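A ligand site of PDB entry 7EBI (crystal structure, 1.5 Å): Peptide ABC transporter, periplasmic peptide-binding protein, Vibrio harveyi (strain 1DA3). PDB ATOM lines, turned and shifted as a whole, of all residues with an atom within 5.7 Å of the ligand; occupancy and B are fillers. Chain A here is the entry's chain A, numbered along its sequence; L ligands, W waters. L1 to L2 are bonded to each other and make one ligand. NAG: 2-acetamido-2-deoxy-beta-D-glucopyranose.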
ATOM      1  N   HIS A   9     -10.332 -11.466  18.209  1.00  0.00           N
ATOM      2  CA  HIS A   9      -9.204 -10.725  17.660  1.00  0.00           C
ATOM      3  C   HIS A   9      -8.627 -11.425  16.436  1.00  0.00           C
ATOM      4  O   HIS A   9      -7.666 -12.181  16.541  1.00  0.00           O
ATOM      5  CB  HIS A   9      -8.145 -10.546  18.746  1.00  0.00           C
ATOM      6  CG  HIS A   9      -6.930  -9.794  18.294  1.00  0.00           C
ATOM      7  ND1 HIS A   9      -6.977  -8.694  17.470  1.00  0.00           N
ATOM      8  CD2 HIS A   9      -5.622  -9.999  18.580  1.00  0.00           C
ATOM      9  CE1 HIS A   9      -5.743  -8.250  17.269  1.00  0.00           C
ATOM     10  NE2 HIS A   9      -4.902  -9.030  17.936  1.00  0.00           N
ATOM     11  N   PRO A  10      -9.223 -11.182  15.269  1.00  0.00           N
ATOM     12  CA  PRO A  10      -8.743 -11.849  14.051  1.00  0.00           C
ATOM     13  C   PRO A  10      -7.484 -11.252  13.418  1.00  0.00           C
ATOM     14  O   PRO A  10      -6.781 -11.979  12.723  1.00  0.00           O
ATOM     15  CB  PRO A  10      -9.922 -11.714  13.077  1.00  0.00           C
ATOM     16  CG  PRO A  10     -10.697 -10.514  13.564  1.00  0.00           C
ATOM     17  CD  PRO A  10     -10.522 -10.509  15.060  1.00  0.00           C
ATOM     18  N   LYS A  11      -7.225  -9.968  13.635  1.00  0.00           N
ATOM     19  CA  LYS A  11      -6.203  -9.280  12.858  1.00  0.00           C
ATOM     20  C   LYS A  11      -5.756  -8.007  13.578  1.00  0.00           C
ATOM     21  O   LYS A  11      -6.583  -7.307  14.134  1.00  0.00           O
ATOM     22  CB  LYS A  11      -6.739  -8.941  11.463  1.00  0.00           C
ATOM     23  CG  LYS A  11      -5.879  -8.040  10.602  1.00  0.00           C
ATOM     24  CD  LYS A  11      -4.651  -8.739  10.082  1.00  0.00           C
ATOM     25  CE  LYS A  11      -3.923  -7.859   9.041  1.00  0.00           C
ATOM     26  NZ  LYS A  11      -2.674  -8.497   8.521  1.00  0.00           N
ATOM     27  N   GLU A  12      -4.458  -7.731  13.561  1.00  0.00           N
ATOM     28  CA  GLU A  12      -3.912  -6.486  14.084  1.00  0.00           C
ATOM     29  C   GLU A  12      -4.267  -5.293  13.214  1.00  0.00           C
ATOM     30  O   GLU A  12      -4.168  -5.359  11.981  1.00  0.00           O
ATOM     31  CB  GLU A  12      -2.402  -6.585  14.167  1.00  0.00           C
ATOM     32  CG  GLU A  12      -1.929  -7.784  14.930  1.00  0.00           C
ATOM     33  CD  GLU A  12      -1.591  -8.999  14.052  1.00  0.00           C
ATOM     34  OE1 GLU A  12      -2.149  -9.182  12.934  1.00  0.00           O
ATOM     35  OE2 GLU A  12      -0.743  -9.790  14.515  1.00  0.00           O
ATOM     36  N   ASN A 206       1.770  -7.856  19.307  1.00  0.00           N
ATOM     37  CA  ASN A 206       1.729  -8.913  20.300  1.00  0.00           C
ATOM     38  C   ASN A 206       1.915  -8.390  21.722  1.00  0.00           C
ATOM     39  O   ASN A 206       1.425  -8.992  22.656  1.00  0.00           O
ATOM     40  CB  ASN A 206       2.784  -9.993  20.012  1.00  0.00           C
ATOM     41  CG  ASN A 206       2.380 -10.906  18.879  1.00  0.00           C
ATOM     42  OD1 ASN A 206       1.252 -10.836  18.359  1.00  0.00           O
ATOM     43  ND2 ASN A 206       3.296 -11.777  18.473  1.00  0.00           N
ATOM     44  N   SER A 222      -6.134 -15.941  18.604  1.00  0.00           N
ATOM     45  CA  SER A 222      -5.226 -16.863  17.927  1.00  0.00           C
ATOM     46  C   SER A 222      -3.869 -16.226  17.735  1.00  0.00           C
ATOM     47  O   SER A 222      -3.193 -16.467  16.741  1.00  0.00           O
ATOM     48  CB  SER A 222      -5.790 -17.270  16.562  1.00  0.00           C
ATOM     49  OG  SER A 222      -6.961 -18.070  16.710  1.00  0.00           O
ATOM     50  N   SER A 223      -3.459 -15.439  18.717  1.00  0.00           N
ATOM     51  CA  SER A 223      -2.177 -14.742  18.651  1.00  0.00           C
ATOM     52  C   SER A 223      -1.032 -15.525  19.274  1.00  0.00           C
ATOM     53  O   SER A 223      -1.232 -16.441  20.078  1.00  0.00           O
ATOM     54  CB  SER A 223      -2.271 -13.393  19.368  1.00  0.00           C
ATOM     55  OG  SER A 223      -3.168 -12.517  18.696  1.00  0.00           O
ATOM     56  N   PHE A 224       0.199 -15.126  18.935  1.00  0.00           N
ATOM     57  CA  PHE A 224       1.342 -15.645  19.647  1.00  0.00           C
ATOM     58  C   PHE A 224       1.387 -15.091  21.061  1.00  0.00           C
ATOM     59  O   PHE A 224       1.269 -13.876  21.267  1.00  0.00           O
ATOM     60  CB  PHE A 224       2.647 -15.308  18.921  1.00  0.00           C
ATOM     61  CG  PHE A 224       3.862 -15.728  19.702  1.00  0.00           C
ATOM     62  CD1 PHE A 224       4.212 -17.069  19.770  1.00  0.00           C
ATOM     63  CD2 PHE A 224       4.629 -14.792  20.378  1.00  0.00           C
ATOM     64  CE1 PHE A 224       5.327 -17.467  20.521  1.00  0.00           C
ATOM     65  CE2 PHE A 224       5.735 -15.179  21.112  1.00  0.00           C
ATOM     66  CZ  PHE A 224       6.085 -16.520  21.180  1.00  0.00           C
ATOM     67  N   GLN A 249       6.921 -22.971   7.881  1.00  0.00           N
ATOM     68  CA  GLN A 249       7.478 -21.616   7.922  1.00  0.00           C
ATOM     69  C   GLN A 249       8.854 -21.678   7.319  1.00  0.00           C
ATOM     70  O   GLN A 249       9.558 -22.669   7.522  1.00  0.00           O
ATOM     71  CB  GLN A 249       7.541 -21.077   9.359  1.00  0.00           C
ATOM     72  CG  GLN A 249       6.165 -21.028  10.008  1.00  0.00           C
ATOM     73  CD  GLN A 249       6.176 -20.449  11.412  1.00  0.00           C
ATOM     74  OE1 GLN A 249       7.170 -19.905  11.868  1.00  0.00           O
ATOM     75  NE2 GLN A 249       5.046 -20.586  12.097  1.00  0.00           N
ATOM     76  N   PHE A 289       9.761 -19.636  19.845  1.00  0.00           N
ATOM     77  CA  PHE A 289       8.396 -20.166  19.942  1.00  0.00           C
ATOM     78  C   PHE A 289       8.128 -20.879  21.256  1.00  0.00           C
ATOM     79  O   PHE A 289       7.065 -21.480  21.401  1.00  0.00           O
ATOM     80  CB  PHE A 289       8.101 -21.097  18.776  1.00  0.00           C
ATOM     81  CG  PHE A 289       8.106 -20.417  17.452  1.00  0.00           C
ATOM     82  CD1 PHE A 289       9.280 -20.273  16.728  1.00  0.00           C
ATOM     83  CD2 PHE A 289       6.939 -19.894  16.914  1.00  0.00           C
ATOM     84  CE1 PHE A 289       9.307 -19.638  15.511  1.00  0.00           C
ATOM     85  CE2 PHE A 289       6.950 -19.254  15.685  1.00  0.00           C
ATOM     86  CZ  PHE A 289       8.133 -19.122  14.978  1.00  0.00           C
ATOM     87  N   GLY A 364       5.271  -6.447  14.806  1.00  0.00           N
ATOM     88  CA  GLY A 364       4.375  -6.923  15.838  1.00  0.00           C
ATOM     89  C   GLY A 364       4.242  -8.430  15.906  1.00  0.00           C
ATOM     90  O   GLY A 364       3.682  -8.945  16.886  1.00  0.00           O
ATOM     91  N   TRP A 365       4.739  -9.143  14.887  1.00  0.00           N
ATOM     92  CA  TRP A 365       4.679 -10.614  14.908  1.00  0.00           C
ATOM     93  C   TRP A 365       5.949 -11.083  15.593  1.00  0.00           C
ATOM     94  O   TRP A 365       6.911 -11.529  14.937  1.00  0.00           O
ATOM     95  CB  TRP A 365       4.575 -11.227  13.509  1.00  0.00           C
ATOM     96  CG  TRP A 365       3.347 -10.888  12.692  1.00  0.00           C
ATOM     97  CD1 TRP A 365       2.519  -9.833  12.856  1.00  0.00           C
ATOM     98  CD2 TRP A 365       2.839 -11.636  11.582  1.00  0.00           C
ATOM     99  NE1 TRP A 365       1.521  -9.857  11.897  1.00  0.00           N
ATOM    100  CE2 TRP A 365       1.707 -10.959  11.100  1.00  0.00           C
ATOM    101  CE3 TRP A 365       3.255 -12.806  10.931  1.00  0.00           C
ATOM    102  CZ2 TRP A 365       0.958 -11.418  10.010  1.00  0.00           C
ATOM    103  CZ3 TRP A 365       2.514 -13.267   9.847  1.00  0.00           C
ATOM    104  CH2 TRP A 365       1.391 -12.573   9.395  1.00  0.00           C
ATOM    105  N   THR A 366       5.968 -10.953  16.904  1.00  0.00           N
ATOM    106  CA  THR A 366       7.202 -11.030  17.659  1.00  0.00           C
ATOM    107  C   THR A 366       7.891 -12.383  17.614  1.00  0.00           C
ATOM    108  O   THR A 366       9.125 -12.460  17.696  1.00  0.00           O
ATOM    109  CB  THR A 366       6.972 -10.607  19.123  1.00  0.00           C
ATOM    110  OG1 THR A 366       5.937 -11.425  19.685  1.00  0.00           O
ATOM    111  CG2 THR A 366       6.550  -9.166  19.195  1.00  0.00           C
ATOM    112  N   ASP A 367       7.128 -13.468  17.470  1.00  0.00           N
ATOM    113  CA  ASP A 367       7.732 -14.780  17.316  1.00  0.00           C
ATOM    114  C   ASP A 367       8.562 -14.828  16.031  1.00  0.00           C
ATOM    115  O   ASP A 367       9.681 -15.388  16.030  1.00  0.00           O
ATOM    116  CB  ASP A 367       6.677 -15.908  17.350  1.00  0.00           C
ATOM    117  CG  ASP A 367       5.461 -15.654  16.462  1.00  0.00           C
ATOM    118  OD1 ASP A 367       5.191 -14.514  16.059  1.00  0.00           O
ATOM    119  OD2 ASP A 367       4.750 -16.656  16.164  1.00  0.00           O
ATOM    120  N   PHE A 368       8.032 -14.252  14.960  1.00  0.00           N
ATOM    121  CA  PHE A 368       8.772 -14.212  13.698  1.00  0.00           C
ATOM    122  C   PHE A 368       9.939 -13.229  13.793  1.00  0.00           C
ATOM    123  O   PHE A 368      11.029 -13.493  13.256  1.00  0.00           O
ATOM    124  CB  PHE A 368       7.868 -13.836  12.534  1.00  0.00           C
ATOM    125  CG  PHE A 368       6.900 -14.920  12.111  1.00  0.00           C
ATOM    126  CD1 PHE A 368       6.600 -15.987  12.927  1.00  0.00           C
ATOM    127  CD2 PHE A 368       6.265 -14.822  10.877  1.00  0.00           C
ATOM    128  CE1 PHE A 368       5.682 -16.961  12.521  1.00  0.00           C
ATOM    129  CE2 PHE A 368       5.354 -15.798  10.477  1.00  0.00           C
ATOM    130  CZ  PHE A 368       5.074 -16.857  11.306  1.00  0.00           C
ATOM    131  N   ASN A 411       5.134 -17.659   7.152  1.00  0.00           N
ATOM    132  CA  ASN A 411       4.355 -18.893   7.220  1.00  0.00           C
ATOM    133  C   ASN A 411       3.521 -19.085   5.965  1.00  0.00           C
ATOM    134  O   ASN A 411       3.462 -18.226   5.085  1.00  0.00           O
ATOM    135  CB  ASN A 411       3.472 -18.916   8.473  1.00  0.00           C
ATOM    136  CG  ASN A 411       2.588 -17.675   8.607  1.00  0.00           C
ATOM    137  OD1 ASN A 411       2.759 -16.676   7.931  1.00  0.00           O
ATOM    138  ND2 ASN A 411       1.638 -17.764   9.522  1.00  0.00           N
ATOM    139  N   TYR A 412       2.865 -20.227   5.894  1.00  0.00           N
ATOM    140  CA  TYR A 412       2.057 -20.590   4.735  1.00  0.00           C
ATOM    141  C   TYR A 412       0.734 -21.178   5.147  1.00  0.00           C
ATOM    142  O   TYR A 412       0.593 -21.670   6.270  1.00  0.00           O
ATOM    143  CB  TYR A 412       2.770 -21.619   3.874  1.00  0.00           C
ATOM    144  CG  TYR A 412       4.061 -21.171   3.251  1.00  0.00           C
ATOM    145  CD1 TYR A 412       5.267 -21.342   3.915  1.00  0.00           C
ATOM    146  CD2 TYR A 412       4.072 -20.580   2.000  1.00  0.00           C
ATOM    147  CE1 TYR A 412       6.452 -20.944   3.342  1.00  0.00           C
ATOM    148  CE2 TYR A 412       5.246 -20.164   1.417  1.00  0.00           C
ATOM    149  CZ  TYR A 412       6.430 -20.367   2.095  1.00  0.00           C
ATOM    150  OH  TYR A 412       7.609 -19.993   1.485  1.00  0.00           O
ATOM    151  N   PHE A 413      -0.204 -21.182   4.203  1.00  0.00           N
ATOM    152  CA  PHE A 413      -1.407 -21.993   4.320  1.00  0.00           C
ATOM    153  C   PHE A 413      -1.065 -23.460   4.498  1.00  0.00           C
ATOM    154  O   PHE A 413      -0.089 -23.947   3.926  1.00  0.00           O
ATOM    155  CB  PHE A 413      -2.285 -21.858   3.065  1.00  0.00           C
ATOM    156  CG  PHE A 413      -2.742 -20.480   2.759  1.00  0.00           C
ATOM    157  CD1 PHE A 413      -3.053 -19.588   3.783  1.00  0.00           C
ATOM    158  CD2 PHE A 413      -2.863 -20.068   1.448  1.00  0.00           C
ATOM    159  CE1 PHE A 413      -3.476 -18.307   3.475  1.00  0.00           C
ATOM    160  CE2 PHE A 413      -3.290 -18.801   1.139  1.00  0.00           C
ATOM    161  CZ  PHE A 413      -3.598 -17.917   2.155  1.00  0.00           C
ATOM    162  N   ARG A 438       1.399 -13.023  -0.714  1.00  0.00           N
ATOM    163  CA  ARG A 438       2.855 -12.996  -0.796  1.00  0.00           C
ATOM    164  C   ARG A 438       3.532 -14.335  -1.095  1.00  0.00           C
ATOM    165  O   ARG A 438       4.717 -14.367  -1.411  1.00  0.00           O
ATOM    166  CB  ARG A 438       3.409 -12.486   0.525  1.00  0.00           C
ATOM    167  CG  ARG A 438       3.083 -13.439   1.670  1.00  0.00           C
ATOM    168  CD  ARG A 438       3.483 -12.824   3.002  1.00  0.00           C
ATOM    169  NE  ARG A 438       3.297 -13.697   4.152  1.00  0.00           N
ATOM    170  CZ  ARG A 438       2.131 -13.877   4.780  1.00  0.00           C
ATOM    171  NH1 ARG A 438       1.034 -13.278   4.321  1.00  0.00           N
ATOM    172  NH2 ARG A 438       2.076 -14.652   5.851  1.00  0.00           N
ATOM    173  N   PHE A 439       2.804 -15.443  -0.951  1.00  0.00           N
ATOM    174  CA  PHE A 439       3.465 -16.722  -0.700  1.00  0.00           C
ATOM    175  C   PHE A 439       4.332 -17.266  -1.826  1.00  0.00           C
ATOM    176  O   PHE A 439       5.322 -17.942  -1.568  1.00  0.00           O
ATOM    177  CB  PHE A 439       2.417 -17.754  -0.320  1.00  0.00           C
ATOM    178  CG  PHE A 439       1.580 -17.333   0.848  1.00  0.00           C
ATOM    179  CD1 PHE A 439       2.134 -17.274   2.122  1.00  0.00           C
ATOM    180  CD2 PHE A 439       0.258 -16.989   0.678  1.00  0.00           C
ATOM    181  CE1 PHE A 439       1.362 -16.862   3.216  1.00  0.00           C
ATOM    182  CE2 PHE A 439      -0.513 -16.576   1.754  1.00  0.00           C
ATOM    183  CZ  PHE A 439       0.048 -16.518   3.017  1.00  0.00           C
ATOM    184  N   MET A 491      -2.199 -21.410  16.744  1.00  0.00           N
ATOM    185  CA  MET A 491      -2.355 -20.793  18.060  1.00  0.00           C
ATOM    186  C   MET A 491      -3.796 -20.424  18.318  1.00  0.00           C
ATOM    187  O   MET A 491      -4.448 -19.823  17.471  1.00  0.00           O
ATOM    188  CB  MET A 491      -1.502 -19.527  18.200  1.00  0.00           C
ATOM    189  CG  MET A 491      -0.044 -19.692  17.840  1.00  0.00           C
ATOM    190  SD  MET A 491       0.297 -19.252  16.115  1.00  0.00           S
ATOM    191  CE  MET A 491      -0.003 -17.482  16.105  1.00  0.00           C
ATOM    192  N   TRP A 515      -8.815 -16.347  12.845  1.00  0.00           N
ATOM    193  CA  TRP A 515      -8.330 -15.604  11.686  1.00  0.00           C
ATOM    194  C   TRP A 515      -9.305 -15.642  10.517  1.00  0.00           C
ATOM    195  O   TRP A 515      -9.985 -16.639  10.302  1.00  0.00           O
ATOM    196  CB  TRP A 515      -7.008 -16.191  11.196  1.00  0.00           C
ATOM    197  CG  TRP A 515      -5.889 -16.249  12.215  1.00  0.00           C
ATOM    198  CD1 TRP A 515      -5.543 -15.291  13.119  1.00  0.00           C
ATOM    199  CD2 TRP A 515      -4.965 -17.318  12.383  1.00  0.00           C
ATOM    200  NE1 TRP A 515      -4.459 -15.710  13.867  1.00  0.00           N
ATOM    201  CE2 TRP A 515      -4.087 -16.946  13.417  1.00  0.00           C
ATOM    202  CE3 TRP A 515      -4.795 -18.556  11.753  1.00  0.00           C
ATOM    203  CZ2 TRP A 515      -3.048 -17.785  13.847  1.00  0.00           C
ATOM    204  CZ3 TRP A 515      -3.767 -19.385  12.184  1.00  0.00           C
ATOM    205  CH2 TRP A 515      -2.909 -18.994  13.219  1.00  0.00           C
ATOM    206  N   ALA A 516      -9.362 -14.565   9.732  1.00  0.00           N
ATOM    207  CA  ALA A 516      -9.976 -14.662   8.417  1.00  0.00           C
ATOM    208  C   ALA A 516      -9.221 -15.722   7.606  1.00  0.00           C
ATOM    209  O   ALA A 516      -8.017 -15.893   7.754  1.00  0.00           O
ATOM    210  CB  ALA A 516      -9.945 -13.300   7.712  1.00  0.00           C
HETATM  211  C1  NAG L   1      -3.105 -14.905   9.091  1.00  0.00           C
HETATM  212  C2  NAG L   1      -1.662 -15.369   9.271  1.00  0.00           C
HETATM  213  C3  NAG L   1      -1.418 -15.515  10.761  1.00  0.00           C
HETATM  214  C4  NAG L   1      -1.695 -14.156  11.433  1.00  0.00           C
HETATM  215  C5  NAG L   1      -3.095 -13.677  11.065  1.00  0.00           C
HETATM  216  C6  NAG L   1      -3.357 -12.308  11.669  1.00  0.00           C
HETATM  217  C7  NAG L   1      -0.804 -16.619   7.355  1.00  0.00           C
HETATM  218  C8  NAG L   1      -0.586 -17.991   6.756  1.00  0.00           C
HETATM  219  N2  NAG L   1      -1.413 -16.613   8.550  1.00  0.00           N
HETATM  220  O1  NAG L   1      -3.445 -14.812   7.720  1.00  0.00           O
HETATM  221  O3  NAG L   1      -0.059 -15.916  10.962  1.00  0.00           O
HETATM  222  O4  NAG L   1      -1.652 -14.300  12.848  1.00  0.00           O
HETATM  223  O5  NAG L   1      -3.231 -13.598   9.658  1.00  0.00           O
HETATM  224  O6  NAG L   1      -2.390 -11.361  11.169  1.00  0.00           O
HETATM  225  O7  NAG L   1      -0.502 -15.584   6.780  1.00  0.00           O
HETATM  226  C1  NAG L   2      -0.506 -13.721  13.445  1.00  0.00           C
HETATM  227  C2  NAG L   2      -0.825 -13.428  14.901  1.00  0.00           C
HETATM  228  C3  NAG L   2       0.444 -12.975  15.623  1.00  0.00           C
HETATM  229  C4  NAG L   2       1.613 -13.923  15.398  1.00  0.00           C
HETATM  230  C5  NAG L   2       1.780 -14.186  13.900  1.00  0.00           C
HETATM  231  C6  NAG L   2       2.879 -15.210  13.595  1.00  0.00           C
HETATM  232  C7  NAG L   2      -3.091 -12.565  15.342  1.00  0.00           C
HETATM  233  C8  NAG L   2      -3.930 -11.314  15.402  1.00  0.00           C
HETATM  234  N2  NAG L   2      -1.833 -12.368  14.962  1.00  0.00           N
HETATM  235  O3  NAG L   2       0.173 -12.902  17.020  1.00  0.00           O
HETATM  236  O4  NAG L   2       2.788 -13.302  15.941  1.00  0.00           O
HETATM  237  O5  NAG L   2       0.535 -14.690  13.399  1.00  0.00           O
HETATM  238  O6  NAG L   2       2.793 -16.411  14.377  1.00  0.00           O
HETATM  239  O7  NAG L   2      -3.544 -13.665  15.640  1.00  0.00           O
HETATM  240  O   HOH W   1      -2.585 -11.200   8.133  1.00  0.00           O
HETATM  241  O   HOH W   2      -5.594 -13.393  17.617  1.00  0.00           O
HETATM  242  O   HOH W   3      -6.115 -14.073   8.126  1.00  0.00           O
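O7 of NAG L2 sits close to O of Ser 222 (3.0 Å).
Residues that only touch the ligand: His 9 (3.5 Å), Pro 10 (3.6 Å), Lys 11 (3.6 Å), Trp 365 (3.4 Å), Phe 368 (3.5 Å), Tyr 412 (3.8 Å), Phe 439 (3.9 Å) and Met 491 (3.5 Å).
Hydrophobic or aromatic side chains within 4 Å of the ligand: His 9, Phe 224, Trp 365, Phe 368, Phe 439, Met 491 and Trp 515.
An oxygen (O6) of NAG L1 sits at hydrogen-bond distance from the side-chain carboxylate (OE1) of Glu 12 (2.8 Å).
The side-chain carboxylate (OD2) of Asp 367 lies within hydrogen-bond range of an oxygen (O6) of NAG L2, at 2.7 Å.
An oxygen (O3) of NAG L2 lies within hydrogen-bond range of the backbone NH (N) of Phe 224 (2.9 Å).
The indole nitrogen of Trp 515 sits at hydrogen-bond distance from an oxygen (O7) of NAG L2 (2.9 Å).
NH2 of Arg 438 is in hydrogen-bond range of O7 of NAG L1 (2.9 Å).
OD1 of Asn 206 sits at hydrogen-bond distance from O3 of NAG L2 (2.7 Å).
OG of Ser 223 lies within hydrogen-bond range of O7 of NAG L2, 3.3 Å away.
The side-chain amide nitrogen (ND2) of Asn 411 sits at hydrogen-bond distance from an oxygen (O3) of NAG L1 (2.9 Å).
The side-chain amide nitrogen (ND2) of Asn 206 lies close to the backbone carbonyl oxygen (O) of Gly 364 (3.3 Å).
The side-chain hydroxyl of Ser 222 lies close to the backbone carbonyl oxygen of Met 491, at 3.2 Å.
NE1 of Trp 515 sits close to O of Ser 222 (3.2 Å).
The side-chain carboxylate of Glu 12 is in hydrogen-bond range of the indole nitrogen of Trp 365.
NH2 of Arg 438 sits at hydrogen-bond distance from OD1 of Asn 411.
The side-chain amide nitrogen (ND2) of Asn 206 lies within hydrogen-bond range of the side-chain hydroxyl (OG1) of Thr 366 (2.9 Å).
Water W3 bridges the backbone carbonyl oxygen of Ala 516 and an oxygen (O1) of NAG L1.
Water W2 lies within hydrogen-bond range of the backbone carbonyl oxygen (O) of His 9 (2.6 Å), the backbone NH (N) of Ser 222 (2.8 Å), the side-chain hydroxyl (OG) of Ser 223 (2.8 Å) and an oxygen (O7) of NAG L2 (2.9 Å).
Water W1 lies within hydrogen-bond range of the side-chain amino group of Lys 11 and an oxygen (O5) of NAG L1.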
